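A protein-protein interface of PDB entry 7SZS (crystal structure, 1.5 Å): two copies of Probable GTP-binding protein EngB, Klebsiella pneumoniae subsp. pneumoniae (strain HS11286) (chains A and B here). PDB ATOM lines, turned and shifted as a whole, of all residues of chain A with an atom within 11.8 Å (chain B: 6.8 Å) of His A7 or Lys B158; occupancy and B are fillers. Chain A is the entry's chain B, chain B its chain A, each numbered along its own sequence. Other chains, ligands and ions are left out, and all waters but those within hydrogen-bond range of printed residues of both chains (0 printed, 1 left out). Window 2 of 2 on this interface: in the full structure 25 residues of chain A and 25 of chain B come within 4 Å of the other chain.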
ATOM      1  N   HIS A   7      27.921 -20.108  19.072  1.00  0.00           N
ATOM      2  CA  HIS A   7      28.539 -20.563  17.830  1.00  0.00           C
ATOM      3  C   HIS A   7      27.538 -20.569  16.679  1.00  0.00           C
ATOM      4  O   HIS A   7      26.338 -20.779  16.895  1.00  0.00           O
ATOM      5  CB  HIS A   7      29.133 -21.956  18.013  1.00  0.00           C
ATOM      6  CG  HIS A   7      30.177 -22.028  19.083  1.00  0.00           C
ATOM      7  ND1 HIS A   7      29.877 -22.285  20.405  1.00  0.00           N
ATOM      8  CD2 HIS A   7      31.522 -21.868  19.030  1.00  0.00           C
ATOM      9  CE1 HIS A   7      30.990 -22.283  21.116  1.00  0.00           C
ATOM     10  NE2 HIS A   7      32.003 -22.036  20.305  1.00  0.00           N
ATOM     11  N   HIS A   8      28.038 -20.349  15.461  1.00  0.00           N
ATOM     12  CA  HIS A   8      27.168 -20.289  14.293  1.00  0.00           C
ATOM     13  C   HIS A   8      26.533 -21.643  14.016  1.00  0.00           C
ATOM     14  O   HIS A   8      27.170 -22.692  14.159  1.00  0.00           O
ATOM     15  CB  HIS A   8      27.934 -19.836  13.047  1.00  0.00           C
ATOM     16  CG  HIS A   8      27.178 -20.060  11.771  1.00  0.00           C
ATOM     17  ND1 HIS A   8      26.198 -19.199  11.323  1.00  0.00           N
ATOM     18  CD2 HIS A   8      27.238 -21.065  10.864  1.00  0.00           C
ATOM     19  CE1 HIS A   8      25.693 -19.659  10.192  1.00  0.00           C
ATOM     20  NE2 HIS A   8      26.308 -20.789   9.889  1.00  0.00           N
ATOM     21  N   MET A   9      25.269 -21.608  13.606  1.00  0.00           N
ATOM     22  CA  MET A   9      24.543 -22.793  13.186  1.00  0.00           C
ATOM     23  C   MET A   9      23.683 -22.447  11.980  1.00  0.00           C
ATOM     24  O   MET A   9      23.378 -21.281  11.717  1.00  0.00           O
ATOM     25  CB  MET A   9      23.664 -23.341  14.313  1.00  0.00           C
ATOM     26  CG  MET A   9      24.453 -23.756  15.528  1.00  0.00           C
ATOM     27  SD  MET A   9      23.400 -24.386  16.840  1.00  0.00           S
ATOM     28  CE  MET A   9      22.995 -25.993  16.161  1.00  0.00           C
ATOM     29  N   LEU A  10      23.285 -23.483  11.253  1.00  0.00           N
ATOM     30  CA  LEU A  10      22.369 -23.326  10.125  1.00  0.00           C
ATOM     31  C   LEU A  10      20.985 -22.933  10.631  1.00  0.00           C
ATOM     32  O   LEU A  10      20.302 -23.742  11.269  1.00  0.00           O
ATOM     33  CB  LEU A  10      22.292 -24.628   9.339  1.00  0.00           C
ATOM     34  CG  LEU A  10      21.252 -24.643   8.220  1.00  0.00           C
ATOM     35  CD1 LEU A  10      21.736 -23.768   7.104  1.00  0.00           C
ATOM     36  CD2 LEU A  10      21.025 -26.068   7.731  1.00  0.00           C
ATOM     37  N   THR A  11      20.564 -21.705  10.336  1.00  0.00           N
ATOM     38  CA  THR A  11      19.276 -21.193  10.802  1.00  0.00           C
ATOM     39  C   THR A  11      18.129 -21.687   9.930  1.00  0.00           C
ATOM     40  O   THR A  11      18.213 -21.668   8.701  1.00  0.00           O
ATOM     41  CB  THR A  11      19.282 -19.666  10.797  1.00  0.00           C
ATOM     42  OG1 THR A  11      20.314 -19.196  11.668  1.00  0.00           O
ATOM     43  CG2 THR A  11      17.947 -19.103  11.248  1.00  0.00           C
ATOM     44  N   ASN A  12      17.048 -22.119  10.577  1.00  0.00           N
ATOM     45  CA  ASN A  12      15.797 -22.421   9.883  1.00  0.00           C
ATOM     46  C   ASN A  12      14.936 -21.169   9.937  1.00  0.00           C
ATOM     47  O   ASN A  12      14.318 -20.863  10.961  1.00  0.00           O
ATOM     48  CB  ASN A  12      15.101 -23.618  10.525  1.00  0.00           C
ATOM     49  CG  ASN A  12      15.941 -24.884  10.475  1.00  0.00           C
ATOM     50  OD1 ASN A  12      16.046 -25.604  11.475  1.00  0.00           O
ATOM     51  ND2 ASN A  12      16.530 -25.174   9.308  1.00  0.00           N
ATOM     52  N   ASN A 207      22.129 -19.338   4.274  1.00  0.00           N
ATOM     53  CA  ASN A 207      23.260 -19.524   5.166  1.00  0.00           C
ATOM     54  C   ASN A 207      24.540 -18.926   4.595  1.00  0.00           C
ATOM     55  O   ASN A 207      25.518 -18.781   5.334  1.00  0.00           O
ATOM     56  CB  ASN A 207      23.427 -21.027   5.436  1.00  0.00           C
ATOM     57  CG  ASN A 207      24.524 -21.330   6.420  1.00  0.00           C
ATOM     58  OD1 ASN A 207      25.512 -21.990   6.080  1.00  0.00           O
ATOM     59  ND2 ASN A 207      24.367 -20.846   7.646  1.00  0.00           N
ATOM     60  N   ASP B 126      20.515 -31.989  27.117  1.00  0.00           N
ATOM     61  CA  ASP B 126      21.634 -31.080  26.886  1.00  0.00           C
ATOM     62  C   ASP B 126      22.758 -31.791  26.139  1.00  0.00           C
ATOM     63  O   ASP B 126      23.242 -32.842  26.573  1.00  0.00           O
ATOM     64  CB  ASP B 126      22.125 -30.557  28.244  1.00  0.00           C
ATOM     65  CG  ASP B 126      23.072 -29.370  28.137  1.00  0.00           C
ATOM     66  OD1 ASP B 126      24.012 -29.393  27.315  1.00  0.00           O
ATOM     67  OD2 ASP B 126      22.884 -28.418  28.920  1.00  0.00           O
ATOM     68  N   ILE B 127      23.186 -31.202  25.017  1.00  0.00           N
ATOM     69  CA  ILE B 127      24.240 -31.809  24.207  1.00  0.00           C
ATOM     70  C   ILE B 127      25.529 -32.026  24.996  1.00  0.00           C
ATOM     71  O   ILE B 127      26.320 -32.906  24.649  1.00  0.00           O
ATOM     72  CB  ILE B 127      24.504 -30.941  22.954  1.00  0.00           C
ATOM     73  CG1 ILE B 127      25.371 -31.704  21.952  1.00  0.00           C
ATOM     74  CG2 ILE B 127      25.144 -29.614  23.354  1.00  0.00           C
ATOM     75  CD1 ILE B 127      25.374 -31.098  20.553  1.00  0.00           C
ATOM     76  N   ARG B 128      25.755 -31.253  26.057  1.00  0.00           N
ATOM     77  CA  ARG B 128      26.973 -31.409  26.846  1.00  0.00           C
ATOM     78  C   ARG B 128      26.895 -32.571  27.820  1.00  0.00           C
ATOM     79  O   ARG B 128      27.944 -33.075  28.241  1.00  0.00           O
ATOM     80  CB  ARG B 128      27.263 -30.119  27.610  1.00  0.00           C
ATOM     81  CG  ARG B 128      27.477 -28.922  26.692  1.00  0.00           C
ATOM     82  CD  ARG B 128      27.442 -27.631  27.467  1.00  0.00           C
ATOM     83  NE  ARG B 128      26.100 -27.355  27.971  1.00  0.00           N
ATOM     84  CZ  ARG B 128      25.797 -26.333  28.761  1.00  0.00           C
ATOM     85  NH1 ARG B 128      26.711 -25.451  29.131  1.00  0.00           N
ATOM     86  NH2 ARG B 128      24.541 -26.179  29.173  1.00  0.00           N
ATOM     87  N   THR B 154      20.062 -30.692  22.828  1.00  0.00           N
ATOM     88  CA  THR B 154      19.687 -29.291  22.918  1.00  0.00           C
ATOM     89  C   THR B 154      20.874 -28.421  23.317  1.00  0.00           C
ATOM     90  O   THR B 154      21.926 -28.904  23.752  1.00  0.00           O
ATOM     91  CB  THR B 154      18.564 -29.096  23.936  1.00  0.00           C
ATOM     92  OG1 THR B 154      18.973 -29.653  25.195  1.00  0.00           O
ATOM     93  CG2 THR B 154      17.277 -29.786  23.469  1.00  0.00           C
ATOM     94  N   LYS B 155      20.670 -27.105  23.182  1.00  0.00           N
ATOM     95  CA  LYS B 155      21.687 -26.107  23.505  1.00  0.00           C
ATOM     96  C   LYS B 155      22.946 -26.334  22.677  1.00  0.00           C
ATOM     97  O   LYS B 155      24.065 -26.062  23.126  1.00  0.00           O
ATOM     98  CB  LYS B 155      21.980 -26.096  25.011  1.00  0.00           C
ATOM     99  CG  LYS B 155      20.691 -26.026  25.850  1.00  0.00           C
ATOM    100  CD  LYS B 155      20.950 -25.888  27.352  1.00  0.00           C
ATOM    101  CE  LYS B 155      19.641 -25.970  28.123  1.00  0.00           C
ATOM    102  NZ  LYS B 155      19.858 -25.851  29.604  1.00  0.00           N
ATOM    103  N   ALA B 156      22.752 -26.812  21.440  1.00  0.00           N
ATOM    104  CA  ALA B 156      23.876 -27.179  20.583  1.00  0.00           C
ATOM    105  C   ALA B 156      24.714 -25.974  20.198  1.00  0.00           C
ATOM    106  O   ALA B 156      25.878 -26.145  19.808  1.00  0.00           O
ATOM    107  CB  ALA B 156      23.369 -27.901  19.329  1.00  0.00           C
ATOM    108  N   ASP B 157      24.169 -24.763  20.335  1.00  0.00           N
ATOM    109  CA  ASP B 157      24.918 -23.527  20.114  1.00  0.00           C
ATOM    110  C   ASP B 157      26.031 -23.304  21.131  1.00  0.00           C
ATOM    111  O   ASP B 157      26.874 -22.425  20.915  1.00  0.00           O
ATOM    112  CB  ASP B 157      23.964 -22.341  20.166  1.00  0.00           C
ATOM    113  CG  ASP B 157      23.177 -22.304  21.458  1.00  0.00           C
ATOM    114  OD1 ASP B 157      22.142 -22.994  21.541  1.00  0.00           O
ATOM    115  OD2 ASP B 157      23.622 -21.623  22.408  1.00  0.00           O
ATOM    116  N   LYS B 158      26.039 -24.049  22.235  1.00  0.00           N
ATOM    117  CA  LYS B 158      27.089 -23.897  23.235  1.00  0.00           C
ATOM    118  C   LYS B 158      28.383 -24.584  22.836  1.00  0.00           C
ATOM    119  O   LYS B 158      29.400 -24.389  23.515  1.00  0.00           O
ATOM    120  CB  LYS B 158      26.602 -24.440  24.578  1.00  0.00           C
ATOM    121  CG  LYS B 158      25.508 -23.592  25.198  1.00  0.00           C
ATOM    122  CD  LYS B 158      25.137 -24.076  26.579  1.00  0.00           C
ATOM    123  CE  LYS B 158      24.196 -23.115  27.298  1.00  0.00           C
ATOM    124  NZ  LYS B 158      24.896 -21.909  27.837  1.00  0.00           N
ATOM    125  N   LEU B 159      28.380 -25.371  21.765  1.00  0.00           N
ATOM    126  CA  LEU B 159      29.573 -26.056  21.288  1.00  0.00           C
ATOM    127  C   LEU B 159      29.939 -25.563  19.898  1.00  0.00           C
ATOM    128  O   LEU B 159      29.057 -25.273  19.082  1.00  0.00           O
ATOM    129  CB  LEU B 159      29.362 -27.570  21.240  1.00  0.00           C
ATOM    130  CG  LEU B 159      29.116 -28.265  22.579  1.00  0.00           C
ATOM    131  CD1 LEU B 159      28.900 -29.749  22.358  1.00  0.00           C
ATOM    132  CD2 LEU B 159      30.257 -28.026  23.557  1.00  0.00           C
ATOM    133  N   ALA B 160      31.242 -25.475  19.633  1.00  0.00           N
ATOM    134  CA  ALA B 160      31.709 -25.240  18.278  1.00  0.00           C
ATOM    135  C   ALA B 160      31.412 -26.456  17.408  1.00  0.00           C
ATOM    136  O   ALA B 160      31.122 -27.549  17.903  1.00  0.00           O
ATOM    137  CB  ALA B 160      33.206 -24.924  18.272  1.00  0.00           C
ATOM    138  N   SER B 161      31.484 -26.255  16.089  1.00  0.00           N
ATOM    139  CA  SER B 161      30.955 -27.253  15.162  1.00  0.00           C
ATOM    140  C   SER B 161      31.639 -28.607  15.332  1.00  0.00           C
ATOM    141  O   SER B 161      30.977 -29.650  15.295  1.00  0.00           O
ATOM    142  CB  SER B 161      31.085 -26.758  13.719  1.00  0.00           C
ATOM    143  OG  SER B 161      32.439 -26.711  13.321  1.00  0.00           O
ATOM    144  N   ARG B 164      30.448 -30.192  18.590  1.00  0.00           N
ATOM    145  CA  ARG B 164      29.044 -30.540  18.415  1.00  0.00           C
ATOM    146  C   ARG B 164      28.901 -31.860  17.665  1.00  0.00           C
ATOM    147  O   ARG B 164      28.147 -32.749  18.083  1.00  0.00           O
ATOM    148  CB  ARG B 164      28.340 -29.409  17.670  1.00  0.00           C
ATOM    149  CG  ARG B 164      26.838 -29.547  17.577  1.00  0.00           C
ATOM    150  CD  ARG B 164      26.278 -28.482  16.649  1.00  0.00           C
ATOM    151  NE  ARG B 164      26.817 -27.169  16.975  1.00  0.00           N
ATOM    152  CZ  ARG B 164      27.095 -26.227  16.084  1.00  0.00           C
ATOM    153  NH1 ARG B 164      26.840 -26.395  14.796  1.00  0.00           N
ATOM    154  NH2 ARG B 164      27.653 -25.092  16.494  1.00  0.00           N
ATOM    155  N   SER B 188      19.080 -26.273  18.499  1.00  0.00           N
ATOM    156  CA  SER B 188      19.225 -25.022  19.247  1.00  0.00           C
ATOM    157  C   SER B 188      17.973 -24.170  19.082  1.00  0.00           C
ATOM    158  O   SER B 188      17.725 -23.631  17.999  1.00  0.00           O
ATOM    159  CB  SER B 188      20.453 -24.239  18.795  1.00  0.00           C
ATOM    160  OG  SER B 188      20.503 -22.979  19.441  1.00  0.00           O
ATOM    161  N   LYS B 191      19.347 -20.439  18.334  1.00  0.00           N
ATOM    162  CA  LYS B 191      19.751 -20.147  16.966  1.00  0.00           C
ATOM    163  C   LYS B 191      18.755 -20.665  15.943  1.00  0.00           C
ATOM    164  O   LYS B 191      19.007 -20.555  14.737  1.00  0.00           O
ATOM    165  CB  LYS B 191      21.139 -20.731  16.693  1.00  0.00           C
ATOM    166  CG  LYS B 191      22.214 -20.220  17.634  1.00  0.00           C
ATOM    167  CD  LYS B 191      22.336 -18.706  17.536  1.00  0.00           C
ATOM    168  CE  LYS B 191      23.517 -18.184  18.343  1.00  0.00           C
ATOM    169  NZ  LYS B 191      23.706 -16.714  18.142  1.00  0.00           N
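CE1 of His A7 touches O of Lys B158 (3.6 Å). Ala B160 touches His A7. His A7 touches Arg B164 (CB to NH2, 3.8 Å). Met A9 touches Ala B156 (CE to CB, 3.7 Å). CG of Met A9 touches NH2 of Arg B164, at 3.6 Å. Met A9 touches Ser B188. Thr A11 touches Lys B191 (OG1 to O, 3.6 Å).
The backbone carbonyl oxygen (O) of Ala B156 is in hydrogen-bond range of the guanidinium group (NE) of Arg B164 (3.2 Å). The side-chain carboxylate (OD1) of Asp B157 is in hydrogen-bond range of the side-chain hydroxyl (OG) of Ser B188 (2.7 Å). The backbone carbonyl oxygen (O) of Leu B159 is in hydrogen-bond range of the guanidinium group (NH2) of Arg B164 (2.9 Å). The backbone NH of Lys B191 sits at hydrogen-bond distance from the side-chain hydroxyl of Ser B188, at 3.0 Å. A ring nitrogen (NE2) of His A8 is in hydrogen-bond range of the side-chain amide nitrogen (ND2) of Asn A207 (3.0 Å).
No position is printed for both chains.
The backbone carbonyl oxygen (O) of Asp B157 is in hydrogen-bond range of a ring nitrogen (ND1) of His A7 (3.0 Å). The backbone NH (N) of Asp B157 lies within hydrogen-bond range of the side-chain sulfur (SD) of Met A9. A ring nitrogen (ND1) of His A7 lies close to the backbone carbonyl oxygen of Leu B159, at 3.4 Å. O of His A8 is in hydrogen-bond range of NH2 of Arg B164.
His A7 touches five residues of chain B. Of the printed residues of chain B, His A8 touches Arg B164. Printed residues of chain B within 4 Å of Met A9: Ala B156, Asp B157, Arg B164 and Ser B188. Of the printed residues of chain B, Thr A11 touches Lys B191. No residue of chain A comes within 4 Å of Lys B155. Ala B156 touches one residue of chain A. Of chain A, only His A7 (3.6 Å) comes within 4 Å of Lys B158. Of the printed residues of chain A, Ser B188 touches Met A9 (3.5 Å). Printed residues of chain A within 4 Å of Lys B191: Thr A11 (3.6 Å).
Printed residues of chain B that touch a printed residue of chain A: Ala B156, Asp B157, Lys B158, Leu B159, Ala B160, Arg B164, Ser B188 and Lys B191. Hydrophobic or aromatic side chains of chain B within 4 Å of the printed part of chain A: Ala B156 and Ala B160. Printed residues of chain A that touch a printed residue of chain B: His A7, His A8, Met A9 and Thr A11. Hydrophobic or aromatic side chains of chain A that line the printed part of chain B: His A7 and Met A9. Along chain A the printed residues that touch a printed residue of chain B span positions 7 to 11. Among the printed residues, no Asp or Glu carboxylate lies within 4 Å of a Lys or Arg side-chain nitrogen of the other chain.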
